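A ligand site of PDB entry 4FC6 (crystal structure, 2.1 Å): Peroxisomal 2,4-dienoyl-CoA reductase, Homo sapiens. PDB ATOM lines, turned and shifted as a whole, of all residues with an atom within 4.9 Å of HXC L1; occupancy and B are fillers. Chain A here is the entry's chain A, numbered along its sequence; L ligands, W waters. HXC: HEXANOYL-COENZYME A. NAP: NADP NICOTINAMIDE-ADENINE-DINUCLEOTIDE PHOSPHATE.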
ATOM      1  N   ARG A  59       6.262 -38.668 -11.106  1.00  0.00           N
ATOM      2  CA  ARG A  59       6.148 -38.285 -12.522  1.00  0.00           C
ATOM      3  C   ARG A  59       6.545 -39.389 -13.513  1.00  0.00           C
ATOM      4  O   ARG A  59       5.870 -39.579 -14.493  1.00  0.00           O
ATOM      5  CB  ARG A  59       6.931 -36.988 -12.839  1.00  0.00           C
ATOM      6  CG  ARG A  59       6.518 -35.755 -12.014  1.00  0.00           C
ATOM      7  CD  ARG A  59       7.581 -34.693 -11.973  1.00  0.00           C
ATOM      8  NE  ARG A  59       8.810 -35.157 -11.301  1.00  0.00           N
ATOM      9  CZ  ARG A  59       9.923 -34.473 -11.238  1.00  0.00           C
ATOM     10  NH1 ARG A  59      10.008 -33.259 -11.831  1.00  0.00           N
ATOM     11  NH2 ARG A  59      10.977 -34.993 -10.632  1.00  0.00           N
ATOM     12  N   ARG A  87       1.527 -31.627  -8.633  1.00  0.00           N
ATOM     13  CA  ARG A  87       1.037 -30.251  -8.916  1.00  0.00           C
ATOM     14  C   ARG A  87      -0.208 -30.227  -9.801  1.00  0.00           C
ATOM     15  O   ARG A  87      -0.753 -29.164 -10.116  1.00  0.00           O
ATOM     16  CB  ARG A  87       2.115 -29.446  -9.611  1.00  0.00           C
ATOM     17  CG  ARG A  87       3.337 -29.226  -8.740  1.00  0.00           C
ATOM     18  CD  ARG A  87       4.472 -28.683  -9.567  1.00  0.00           C
ATOM     19  NE  ARG A  87       5.071 -29.750 -10.389  1.00  0.00           N
ATOM     20  CZ  ARG A  87       6.275 -29.672 -10.974  1.00  0.00           C
ATOM     21  NH1 ARG A  87       6.987 -28.542 -10.875  1.00  0.00           N
ATOM     22  NH2 ARG A  87       6.758 -30.712 -11.662  1.00  0.00           N
ATOM     23  N   ALA A 114       9.155 -34.645  -3.534  1.00  0.00           N
ATOM     24  CA  ALA A 114       9.829 -33.360  -3.253  1.00  0.00           C
ATOM     25  C   ALA A 114      10.861 -33.076  -4.320  1.00  0.00           C
ATOM     26  O   ALA A 114      11.243 -33.964  -5.045  1.00  0.00           O
ATOM     27  CB  ALA A 114      10.519 -33.367  -1.894  1.00  0.00           C
ATOM     28  N   GLY A 115      11.361 -31.840  -4.319  1.00  0.00           N
ATOM     29  CA  GLY A 115      12.450 -31.406  -5.191  1.00  0.00           C
ATOM     30  C   GLY A 115      13.431 -30.536  -4.422  1.00  0.00           C
ATOM     31  O   GLY A 115      13.057 -29.717  -3.540  1.00  0.00           O
ATOM     32  N   ASN A 116      14.707 -30.673  -4.721  1.00  0.00           N
ATOM     33  CA  ASN A 116      15.727 -29.883  -4.032  1.00  0.00           C
ATOM     34  C   ASN A 116      17.046 -29.847  -4.767  1.00  0.00           C
ATOM     35  O   ASN A 116      17.307 -30.654  -5.654  1.00  0.00           O
ATOM     36  CB  ASN A 116      15.922 -30.408  -2.608  1.00  0.00           C
ATOM     37  CG  ASN A 116      16.494 -29.363  -1.630  1.00  0.00           C
ATOM     38  OD1 ASN A 116      16.860 -28.226  -1.990  1.00  0.00           O
ATOM     39  ND2 ASN A 116      16.592 -29.764  -0.369  1.00  0.00           N
ATOM     40  N   PHE A 117      17.890 -28.896  -4.352  1.00  0.00           N
ATOM     41  CA  PHE A 117      19.191 -28.628  -4.972  1.00  0.00           C
ATOM     42  C   PHE A 117      19.804 -27.520  -4.133  1.00  0.00           C
ATOM     43  O   PHE A 117      19.096 -26.794  -3.420  1.00  0.00           O
ATOM     44  CB  PHE A 117      19.056 -28.209  -6.463  1.00  0.00           C
ATOM     45  CG  PHE A 117      18.023 -27.124  -6.708  1.00  0.00           C
ATOM     46  CD1 PHE A 117      18.302 -25.797  -6.473  1.00  0.00           C
ATOM     47  CD2 PHE A 117      16.747 -27.463  -7.160  1.00  0.00           C
ATOM     48  CE1 PHE A 117      17.322 -24.792  -6.689  1.00  0.00           C
ATOM     49  CE2 PHE A 117      15.792 -26.502  -7.365  1.00  0.00           C
ATOM     50  CZ  PHE A 117      16.066 -25.158  -7.127  1.00  0.00           C
ATOM     51  N   LEU A 118      21.126 -27.386  -4.175  1.00  0.00           N
ATOM     52  CA  LEU A 118      21.808 -26.303  -3.449  1.00  0.00           C
ATOM     53  C   LEU A 118      21.799 -25.050  -4.316  1.00  0.00           C
ATOM     54  O   LEU A 118      22.075 -25.136  -5.511  1.00  0.00           O
ATOM     55  CB  LEU A 118      23.227 -26.719  -3.140  1.00  0.00           C
ATOM     56  CG  LEU A 118      23.334 -27.822  -2.112  1.00  0.00           C
ATOM     57  CD1 LEU A 118      24.837 -28.137  -2.089  1.00  0.00           C
ATOM     58  CD2 LEU A 118      22.804 -27.338  -0.743  1.00  0.00           C
ATOM     59  N   CYS A 119      21.425 -23.893  -3.762  1.00  0.00           N
ATOM     60  CA  CYS A 119      21.549 -22.658  -4.547  1.00  0.00           C
ATOM     61  C   CYS A 119      21.533 -21.472  -3.584  1.00  0.00           C
ATOM     62  O   CYS A 119      20.686 -21.415  -2.709  1.00  0.00           O
ATOM     63  CB  CYS A 119      20.415 -22.503  -5.568  1.00  0.00           C
ATOM     64  SG  CYS A 119      20.612 -21.095  -6.694  1.00  0.00           S
ATOM     65  N   LEU A 124      19.110 -17.682  -6.781  1.00  0.00           N
ATOM     66  CA  LEU A 124      17.942 -18.505  -7.070  1.00  0.00           C
ATOM     67  C   LEU A 124      16.916 -17.702  -7.810  1.00  0.00           C
ATOM     68  O   LEU A 124      16.604 -16.544  -7.429  1.00  0.00           O
ATOM     69  CB  LEU A 124      17.355 -18.951  -5.743  1.00  0.00           C
ATOM     70  CG  LEU A 124      16.132 -19.883  -5.728  1.00  0.00           C
ATOM     71  CD1 LEU A 124      16.638 -21.276  -6.159  1.00  0.00           C
ATOM     72  CD2 LEU A 124      15.588 -19.958  -4.285  1.00  0.00           C
ATOM     73  N   SER A 125      16.410 -18.245  -8.910  1.00  0.00           N
ATOM     74  CA  SER A 125      15.453 -17.459  -9.688  1.00  0.00           C
ATOM     75  C   SER A 125      14.074 -17.546  -9.051  1.00  0.00           C
ATOM     76  O   SER A 125      13.775 -18.412  -8.227  1.00  0.00           O
ATOM     77  CB  SER A 125      15.399 -17.975 -11.139  1.00  0.00           C
ATOM     78  OG  SER A 125      14.750 -19.249 -11.162  1.00  0.00           O
ATOM     79  N   ASN A 127      11.304 -18.491 -10.455  1.00  0.00           N
ATOM     80  CA  ASN A 127      10.662 -19.759 -10.834  1.00  0.00           C
ATOM     81  C   ASN A 127      11.272 -20.967 -10.068  1.00  0.00           C
ATOM     82  O   ASN A 127      10.562 -21.892  -9.747  1.00  0.00           O
ATOM     83  CB  ASN A 127      10.717 -19.973 -12.354  1.00  0.00           C
ATOM     84  CG  ASN A 127       9.978 -21.232 -12.784  1.00  0.00           C
ATOM     85  OD1 ASN A 127       8.857 -21.450 -12.369  1.00  0.00           O
ATOM     86  ND2 ASN A 127      10.588 -22.043 -13.681  1.00  0.00           N
ATOM     87  N   ALA A 128      12.576 -20.968  -9.806  1.00  0.00           N
ATOM     88  CA  ALA A 128      13.190 -22.040  -9.006  1.00  0.00           C
ATOM     89  C   ALA A 128      12.612 -22.062  -7.579  1.00  0.00           C
ATOM     90  O   ALA A 128      12.242 -23.101  -7.068  1.00  0.00           O
ATOM     91  CB  ALA A 128      14.684 -21.883  -8.959  1.00  0.00           C
ATOM     92  N   THR A 131       8.868 -23.293  -7.909  1.00  0.00           N
ATOM     93  CA  THR A 131       8.766 -24.723  -8.261  1.00  0.00           C
ATOM     94  C   THR A 131       8.925 -25.617  -6.994  1.00  0.00           C
ATOM     95  O   THR A 131       8.209 -26.576  -6.818  1.00  0.00           O
ATOM     96  CB  THR A 131       9.867 -25.089  -9.307  1.00  0.00           C
ATOM     97  OG1 THR A 131       9.638 -24.313 -10.485  1.00  0.00           O
ATOM     98  CG2 THR A 131       9.783 -26.526  -9.666  1.00  0.00           C
ATOM     99  N   VAL A 132       9.905 -25.310  -6.141  1.00  0.00           N
ATOM    100  CA  VAL A 132      10.099 -26.069  -4.900  1.00  0.00           C
ATOM    101  C   VAL A 132       8.859 -25.945  -4.033  1.00  0.00           C
ATOM    102  O   VAL A 132       8.322 -26.969  -3.658  1.00  0.00           O
ATOM    103  CB  VAL A 132      11.427 -25.712  -4.185  1.00  0.00           C
ATOM    104  CG1 VAL A 132      11.586 -26.520  -2.878  1.00  0.00           C
ATOM    105  CG2 VAL A 132      12.575 -26.038  -5.127  1.00  0.00           C
ATOM    106  N   ILE A 135       5.988 -28.142  -5.561  1.00  0.00           N
ATOM    107  CA  ILE A 135       6.131 -29.596  -5.487  1.00  0.00           C
ATOM    108  C   ILE A 135       5.898 -29.989  -4.047  1.00  0.00           C
ATOM    109  O   ILE A 135       5.030 -30.818  -3.772  1.00  0.00           O
ATOM    110  CB  ILE A 135       7.530 -30.133  -5.919  1.00  0.00           C
ATOM    111  CG1 ILE A 135       7.734 -30.049  -7.416  1.00  0.00           C
ATOM    112  CG2 ILE A 135       7.664 -31.602  -5.565  1.00  0.00           C
ATOM    113  CD1 ILE A 135       7.114 -28.837  -8.025  1.00  0.00           C
ATOM    114  N   ALA A 164      11.595 -31.782   6.878  1.00  0.00           N
ATOM    115  CA  ALA A 164      13.050 -31.526   6.967  1.00  0.00           C
ATOM    116  C   ALA A 164      13.248 -30.697   8.206  1.00  0.00           C
ATOM    117  O   ALA A 164      12.251 -30.254   8.772  1.00  0.00           O
ATOM    118  CB  ALA A 164      13.548 -30.762   5.733  1.00  0.00           C
ATOM    119  N   LEU A 166      15.608 -28.185   7.777  1.00  0.00           N
ATOM    120  CA  LEU A 166      16.288 -27.062   7.122  1.00  0.00           C
ATOM    121  C   LEU A 166      15.830 -25.695   7.578  1.00  0.00           C
ATOM    122  O   LEU A 166      16.636 -24.822   7.784  1.00  0.00           O
ATOM    123  CB  LEU A 166      16.128 -27.123   5.589  1.00  0.00           C
ATOM    124  CG  LEU A 166      16.702 -28.353   4.919  1.00  0.00           C
ATOM    125  CD1 LEU A 166      16.162 -28.494   3.499  1.00  0.00           C
ATOM    126  CD2 LEU A 166      18.226 -28.237   4.937  1.00  0.00           C
ATOM    127  N   GLN A 174      19.524 -23.212   0.936  1.00  0.00           N
ATOM    128  CA  GLN A 174      18.334 -23.993   1.011  1.00  0.00           C
ATOM    129  C   GLN A 174      17.084 -23.174   1.296  1.00  0.00           C
ATOM    130  O   GLN A 174      16.130 -23.725   1.861  1.00  0.00           O
ATOM    131  CB  GLN A 174      18.485 -25.083   2.075  1.00  0.00           C
ATOM    132  CG  GLN A 174      19.506 -26.152   1.780  1.00  0.00           C
ATOM    133  CD  GLN A 174      18.984 -27.112   0.768  1.00  0.00           C
ATOM    134  OE1 GLN A 174      18.944 -26.814  -0.459  1.00  0.00           O
ATOM    135  NE2 GLN A 174      18.505 -28.225   1.246  1.00  0.00           N
ATOM    136  N   ALA A 177      13.901 -24.987  -0.097  1.00  0.00           N
ATOM    137  CA  ALA A 177      13.478 -26.228   0.531  1.00  0.00           C
ATOM    138  C   ALA A 177      13.104 -26.034   1.994  1.00  0.00           C
ATOM    139  O   ALA A 177      12.133 -26.653   2.495  1.00  0.00           O
ATOM    140  CB  ALA A 177      14.551 -27.298   0.383  1.00  0.00           C
ATOM    141  N   LYS A 181       9.267 -26.887   3.358  1.00  0.00           N
ATOM    142  CA  LYS A 181       9.074 -27.947   4.346  1.00  0.00           C
ATOM    143  C   LYS A 181       8.500 -27.392   5.689  1.00  0.00           C
ATOM    144  O   LYS A 181       7.683 -28.055   6.370  1.00  0.00           O
ATOM    145  CB  LYS A 181      10.390 -28.713   4.565  1.00  0.00           C
ATOM    146  CG  LYS A 181      10.857 -29.569   3.374  1.00  0.00           C
ATOM    147  CD  LYS A 181       9.927 -30.694   2.953  1.00  0.00           C
ATOM    148  CE  LYS A 181      10.681 -31.678   2.028  1.00  0.00           C
ATOM    149  NZ  LYS A 181       9.944 -32.943   1.689  1.00  0.00           N
ATOM    150  N   GLU A 214      19.139 -39.717  -3.512  1.00  0.00           N
ATOM    151  CA  GLU A 214      19.328 -38.536  -4.342  1.00  0.00           C
ATOM    152  C   GLU A 214      19.524 -37.228  -3.519  1.00  0.00           C
ATOM    153  O   GLU A 214      20.409 -36.380  -3.847  1.00  0.00           O
ATOM    154  CB  GLU A 214      18.147 -38.412  -5.290  1.00  0.00           C
ATOM    155  CG  GLU A 214      18.253 -37.341  -6.356  1.00  0.00           C
ATOM    156  CD  GLU A 214      19.485 -37.467  -7.266  1.00  0.00           C
ATOM    157  OE1 GLU A 214      20.148 -38.521  -7.317  1.00  0.00           O
ATOM    158  OE2 GLU A 214      19.789 -36.453  -7.934  1.00  0.00           O
ATOM    159  N   GLY A 215      18.697 -37.048  -2.456  1.00  0.00           N
ATOM    160  CA  GLY A 215      18.908 -35.881  -1.590  1.00  0.00           C
ATOM    161  C   GLY A 215      20.352 -35.832  -1.071  1.00  0.00           C
ATOM    162  O   GLY A 215      21.024 -34.806  -1.165  1.00  0.00           O
ATOM    163  N   ARG A 218      22.792 -35.022  -4.011  1.00  0.00           N
ATOM    164  CA  ARG A 218      22.693 -33.677  -4.529  1.00  0.00           C
ATOM    165  C   ARG A 218      23.180 -32.595  -3.590  1.00  0.00           C
ATOM    166  O   ARG A 218      23.582 -31.505  -4.014  1.00  0.00           O
ATOM    167  CB  ARG A 218      21.225 -33.360  -4.789  1.00  0.00           C
ATOM    168  CG  ARG A 218      20.725 -33.888  -6.098  1.00  0.00           C
ATOM    169  CD  ARG A 218      19.396 -33.230  -6.391  1.00  0.00           C
ATOM    170  NE  ARG A 218      18.815 -33.845  -7.553  1.00  0.00           N
ATOM    171  CZ  ARG A 218      17.958 -33.234  -8.356  1.00  0.00           C
ATOM    172  NH1 ARG A 218      17.571 -31.985  -8.117  1.00  0.00           N
ATOM    173  NH2 ARG A 218      17.495 -33.895  -9.392  1.00  0.00           N
ATOM    174  N   LEU A 219      23.057 -32.838  -2.308  1.00  0.00           N
ATOM    175  CA  LEU A 219      23.091 -31.720  -1.361  1.00  0.00           C
ATOM    176  C   LEU A 219      24.107 -31.954  -0.308  1.00  0.00           C
ATOM    177  O   LEU A 219      24.341 -31.069   0.495  1.00  0.00           O
ATOM    178  CB  LEU A 219      21.736 -31.560  -0.628  1.00  0.00           C
ATOM    179  CG  LEU A 219      20.416 -31.499  -1.372  1.00  0.00           C
ATOM    180  CD1 LEU A 219      19.378 -32.027  -0.387  1.00  0.00           C
ATOM    181  CD2 LEU A 219      20.067 -30.097  -1.852  1.00  0.00           C
HETATM  182  C2  HXC L   1      19.689 -23.522  -9.193  1.00  0.00           C
HETATM  183  C4  HXC L   1      17.965 -24.622 -10.222  1.00  0.00           C
HETATM  184  C5  HXC L   1      18.673 -25.899  -9.991  1.00  0.00           C
HETATM  185  C6  HXC L   1      19.959 -25.868  -9.321  1.00  0.00           C
HETATM  186  C8  HXC L   1      16.807 -26.283 -11.055  1.00  0.00           C
HETATM  187  N9  HXC L   1      16.853 -24.942 -10.866  1.00  0.00           N
HETATM  188  N7  HXC L   1      17.915 -26.880 -10.528  1.00  0.00           N
HETATM  189  N3  HXC L   1      18.495 -23.457  -9.806  1.00  0.00           N
HETATM  190  N1  HXC L   1      20.358 -24.630  -8.948  1.00  0.00           N
HETATM  191  N6  HXC L   1      20.648 -27.019  -9.078  1.00  0.00           N
HETATM  192  C1' HXC L   1      15.820 -23.989 -11.323  1.00  0.00           C
HETATM  193  C2' HXC L   1      15.706 -24.062 -12.844  1.00  0.00           C
HETATM  194  O2' HXC L   1      16.795 -23.367 -13.478  1.00  0.00           O
HETATM  195  C3' HXC L   1      14.321 -23.446 -13.130  1.00  0.00           C
HETATM  196  O3' HXC L   1      14.450 -22.015 -13.059  1.00  0.00           O
HETATM  197  C4' HXC L   1      13.510 -23.931 -11.917  1.00  0.00           C
HETATM  198  O4' HXC L   1      14.482 -24.309 -10.957  1.00  0.00           O
HETATM  199  C5' HXC L   1      12.583 -25.108 -12.264  1.00  0.00           C
HETATM  200  O5' HXC L   1      13.342 -26.179 -12.925  1.00  0.00           O
HETATM  201  P1  HXC L   1      12.621 -27.265 -13.872  1.00  0.00           P
HETATM  202  O11 HXC L   1      11.856 -26.505 -14.847  1.00  0.00           O
HETATM  203  O12 HXC L   1      13.473 -28.406 -14.289  1.00  0.00           O
HETATM  204  O6  HXC L   1      11.573 -27.765 -12.720  1.00  0.00           O
HETATM  205  P2  HXC L   1      10.871 -29.228 -12.556  1.00  0.00           P
HETATM  206  O21 HXC L   1      10.835 -29.905 -13.860  1.00  0.00           O
HETATM  207  O22 HXC L   1       9.480 -28.951 -12.028  1.00  0.00           O
HETATM  208  O7  HXC L   1      11.889 -30.042 -11.506  1.00  0.00           O
HETATM  209  CPB HXC L   1      11.864 -30.022 -10.051  1.00  0.00           C
HETATM  210  CPA HXC L   1      13.263 -29.839  -9.455  1.00  0.00           C
HETATM  211  CP7 HXC L   1      14.182 -31.009  -9.878  1.00  0.00           C
HETATM  212  CP9 HXC L   1      13.195 -29.635  -7.930  1.00  0.00           C
HETATM  213  CP8 HXC L   1      13.860 -28.536  -9.970  1.00  0.00           C
HETATM  214  OP3 HXC L   1      15.534 -30.823  -9.471  1.00  0.00           O
HETATM  215  CP6 HXC L   1      13.696 -32.384  -9.444  1.00  0.00           C
HETATM  216  OP2 HXC L   1      12.916 -32.867 -10.194  1.00  0.00           O
HETATM  217  NP2 HXC L   1      14.094 -33.008  -8.316  1.00  0.00           N
HETATM  218  CP5 HXC L   1      13.611 -34.305  -7.834  1.00  0.00           C
HETATM  219  CP4 HXC L   1      14.720 -35.060  -7.097  1.00  0.00           C
HETATM  220  CP3 HXC L   1      15.213 -34.325  -5.894  1.00  0.00           C
HETATM  221  OP1 HXC L   1      15.189 -33.112  -5.948  1.00  0.00           O
HETATM  222  NP1 HXC L   1      15.615 -35.086  -4.857  1.00  0.00           N
HETATM  223  CP2 HXC L   1      16.499 -34.784  -3.748  1.00  0.00           C
HETATM  224  CP1 HXC L   1      16.044 -33.657  -2.854  1.00  0.00           C
HETATM  225  S   HXC L   1      14.418 -33.836  -2.185  1.00  0.00           S
HETATM  226  P3  HXC L   1      14.307 -20.961 -14.312  1.00  0.00           P
HETATM  227  O31 HXC L   1      12.929 -21.149 -14.832  1.00  0.00           O
HETATM  228  O32 HXC L   1      14.487 -19.657 -13.575  1.00  0.00           O
HETATM  229  O33 HXC L   1      15.477 -21.392 -15.121  1.00  0.00           O
HETATM  230  CM1 HXC L   1      14.976 -32.982  -0.638  1.00  0.00           C
HETATM  231  CM2 HXC L   1      16.359 -33.124   0.078  1.00  0.00           C
HETATM  232  CM3 HXC L   1      16.346 -32.943   1.618  1.00  0.00           C
HETATM  233  OM2 HXC L   1      14.314 -32.138   0.059  1.00  0.00           O
HETATM  234  CM4 HXC L   1      17.390 -32.014   2.354  1.00  0.00           C
HETATM  235  CM5 HXC L   1      17.438 -32.050   3.916  1.00  0.00           C
HETATM  236  CM6 HXC L   1      18.815 -32.014   4.608  1.00  0.00           C
HETATM  237  PA  NAP L   2      14.386 -38.818  -4.267  1.00  0.00           P
HETATM  238  O1A NAP L   2      14.725 -37.884  -5.475  1.00  0.00           O
HETATM  239  O2A NAP L   2      14.746 -40.255  -4.393  1.00  0.00           O
HETATM  240  O5B NAP L   2      12.809 -38.778  -4.005  1.00  0.00           O
HETATM  241  C5B NAP L   2      12.009 -37.693  -4.425  1.00  0.00           C
HETATM  242  C4B NAP L   2      10.885 -38.323  -5.242  1.00  0.00           C
HETATM  243  O4B NAP L   2       9.907 -37.305  -5.544  1.00  0.00           O
HETATM  244  C3B NAP L   2      11.350 -38.924  -6.563  1.00  0.00           C
HETATM  245  O3B NAP L   2      10.910 -40.308  -6.517  1.00  0.00           O
HETATM  246  C2B NAP L   2      10.573 -38.155  -7.625  1.00  0.00           C
HETATM  247  O2B NAP L   2      10.161 -38.998  -8.689  1.00  0.00           O
HETATM  248  C1B NAP L   2       9.394 -37.567  -6.832  1.00  0.00           C
HETATM  249  N9A NAP L   2       8.896 -36.296  -7.367  1.00  0.00           N
HETATM  250  C8A NAP L   2       9.612 -35.159  -7.554  1.00  0.00           C
HETATM  251  N7A NAP L   2       8.806 -34.193  -8.076  1.00  0.00           N
HETATM  252  C5A NAP L   2       7.554 -34.724  -8.213  1.00  0.00           C
HETATM  253  C6A NAP L   2       6.239 -34.272  -8.679  1.00  0.00           C
HETATM  254  N6A NAP L   2       6.066 -33.025  -9.131  1.00  0.00           N
HETATM  255  N1A NAP L   2       5.192 -35.136  -8.629  1.00  0.00           N
HETATM  256  C2A NAP L   2       5.325 -36.372  -8.176  1.00  0.00           C
HETATM  257  N3A NAP L   2       6.494 -36.864  -7.749  1.00  0.00           N
HETATM  258  C4A NAP L   2       7.600 -36.082  -7.703  1.00  0.00           C
HETATM  259  O3  NAP L   2      15.039 -38.100  -2.971  1.00  0.00           O
HETATM  260  PN  NAP L   2      15.185 -38.597  -1.419  1.00  0.00           P
HETATM  261  O1N NAP L   2      16.461 -38.007  -0.905  1.00  0.00           O
HETATM  262  O2N NAP L   2      14.871 -40.027  -1.151  1.00  0.00           O
HETATM  263  O5D NAP L   2      14.031 -37.702  -0.735  1.00  0.00           O
HETATM  264  C5D NAP L   2      12.708 -38.191  -0.464  1.00  0.00           C
HETATM  265  C4D NAP L   2      12.032 -37.378   0.622  1.00  0.00           C
HETATM  266  O4D NAP L   2      12.814 -37.291   1.799  1.00  0.00           O
HETATM  267  C3D NAP L   2      11.823 -35.957   0.160  1.00  0.00           C
HETATM  268  O3D NAP L   2      10.567 -35.431   0.692  1.00  0.00           O
HETATM  269  C2D NAP L   2      12.993 -35.194   0.738  1.00  0.00           C
HETATM  270  O2D NAP L   2      12.758 -33.804   0.848  1.00  0.00           O
HETATM  271  C1D NAP L   2      13.068 -35.876   2.093  1.00  0.00           C
HETATM  272  N1N NAP L   2      14.365 -35.684   2.763  1.00  0.00           N
HETATM  273  C2N NAP L   2      15.471 -36.425   2.372  1.00  0.00           C
HETATM  274  C3N NAP L   2      16.687 -36.291   3.036  1.00  0.00           C
HETATM  275  C7N NAP L   2      17.903 -37.067   2.559  1.00  0.00           C
HETATM  276  O7N NAP L   2      18.890 -36.907   3.228  1.00  0.00           O
HETATM  277  N7N NAP L   2      17.896 -37.833   1.418  1.00  0.00           N
HETATM  278  C4N NAP L   2      16.766 -35.393   4.158  1.00  0.00           C
HETATM  279  C5N NAP L   2      15.595 -34.645   4.576  1.00  0.00           C
HETATM  280  C6N NAP L   2      14.414 -34.812   3.835  1.00  0.00           C
HETATM  281  P2B NAP L   2       9.732 -38.567 -10.208  1.00  0.00           P
HETATM  282  O1X NAP L   2      10.998 -37.921 -10.657  1.00  0.00           O
HETATM  283  O2X NAP L   2       9.360 -39.880 -10.880  1.00  0.00           O
HETATM  284  O3X NAP L   2       8.539 -37.625 -10.074  1.00  0.00           O
HETATM  285  O   HOH W   1      15.831 -33.218 -11.556  1.00  0.00           O
HETATM  286  O   HOH W   2       9.433 -29.805 -16.827  1.00  0.00           O
HETATM  287  O   HOH W   3      20.093 -29.906  -9.856  1.00  0.00           O
HETATM  288  O   HOH W   4       8.636 -31.704 -13.763  1.00  0.00           O
HETATM  289  O   HOH W   5      12.334 -17.294 -12.786  1.00  0.00           O
HETATM  290  O   HOH W   6      13.183 -37.172  -9.495  1.00  0.00           O
HETATM  291  O   HOH W   7      12.683 -29.928  -0.937  1.00  0.00           O
HETATM  292  O   HOH W   8      11.860 -18.992 -15.600  1.00  0.00           O
HETATM  293  O   HOH W   9      17.434 -29.699 -10.690  1.00  0.00           O
HETATM  294  O   HOH W  10      20.307 -34.143   2.662  1.00  0.00           O
HETATM  295  O   HOH W  11      17.835 -20.686 -10.176  1.00  0.00           O
HETATM  296  O   HOH W  12      15.864 -17.833 -14.821  1.00  0.00           O
HETATM  297  O   HOH W  13      22.723 -23.854  -8.238  1.00  0.00           O
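Water W9 lies within hydrogen-bond range of an oxygen (OP3) of HXC L1 (2.5 Å) and the guanidinium group of Arg 218 (3.4 Å).
Water W13 bridges a nitrogen (N1) of HXC L1 (2.6 Å) and the backbone carbonyl oxygen of Leu 118 (3.1 Å).
Water W11 bridges N3 of HXC L1 (2.9 Å) and N of Ser 125 (3.1 Å).
Water W7 bridges the backbone carbonyl oxygen (O) of Gly 115 (2.6 Å) and an oxygen (OM2) of HXC L1 (2.9 Å).
Water W1 lies within hydrogen-bond range of NH2 of Arg 218 and OP3 of HXC L1.
Water W6 lies within hydrogen-bond range of an oxygen (O1X) of NAP L2 (2.6 Å) and the guanidinium group of Arg 59 (3.3 Å).
OG of Ser 125 lies within hydrogen-bond range of O32 of HXC L1 (2.5 Å).
NH1 of Arg 218 sits at hydrogen-bond distance from OP3 of HXC L1, 2.7 Å away.
The side-chain amide nitrogen (ND2) of Asn 127 sits at hydrogen-bond distance from an oxygen (O31) of HXC L1, at 2.8 Å.
The backbone NH (N) of Asn 116 is in hydrogen-bond range of an oxygen (OP1) of HXC L1 (2.8 Å).
The side-chain amide nitrogen (ND2) of Asn 116 is in hydrogen-bond range of an oxygen (OM2) of HXC L1 (3.3 Å).
NH1 of Arg 87 lies within salt-bridge range of O22 of HXC L1 (2.8 Å).
OP2 of HXC L1 is in hydrogen-bond range of NH2 of Arg 59 (2.9 Å).
N of Arg 59 sits at hydrogen-bond distance from O3X of NAP L2 (2.7 Å).
NE of Arg 59 lies within salt-bridge range of O3X of NAP L2 (2.8 Å).
N of Gly 215 lies within hydrogen-bond range of O1N of NAP L2, 2.9 Å away.
The backbone NH of Ala 114 sits at hydrogen-bond distance from an oxygen (O4B) of NAP L2, 3.4 Å away.
NZ of Lys 181 sits at hydrogen-bond distance from O3D of NAP L2 (2.8 Å).
OM2 of HXC L1 is in hydrogen-bond range of O2D of NAP L2.
Residues that only touch HXC L1: Ala 128, Leu 219, Phe 117, Gly 115, Thr 131, Gly 215, Cys 119, Ala 114, Glu 214, Leu 166 and Leu 118.
17 residues have an atom within 4 Å of HXC L1: Arg 59, Arg 87, Ala 114, Gly 115, Asn 116, Phe 117, Leu 118, Cys 119, Ser 125, Asn 127, Ala 128, Thr 131, Leu 166, Glu 214, Gly 215, Arg 218 and Leu 219.
N of Ala 128 sits at hydrogen-bond distance from OG of Ser 125, 3.1 Å away.
NH1 of Arg 218 sits at hydrogen-bond distance from O of Asn 116.
NE of Arg 218 lies within salt-bridge range of OE2 of Glu 214 (2.8 Å).
The side-chain hydroxyl of Thr 131 lies within hydrogen-bond range of the backbone carbonyl oxygen of Asn 127, at 2.7 Å.
NE2 of Gln 174 lies close to ND2 of Asn 116.
The side-chain amide oxygen (OE1) of Gln 174 lies close to the backbone carbonyl oxygen (O) of Phe 117, at 3.0 Å.
The backbone NH of Leu 124 sits at hydrogen-bond distance from the side-chain sulfur of Cys 119.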
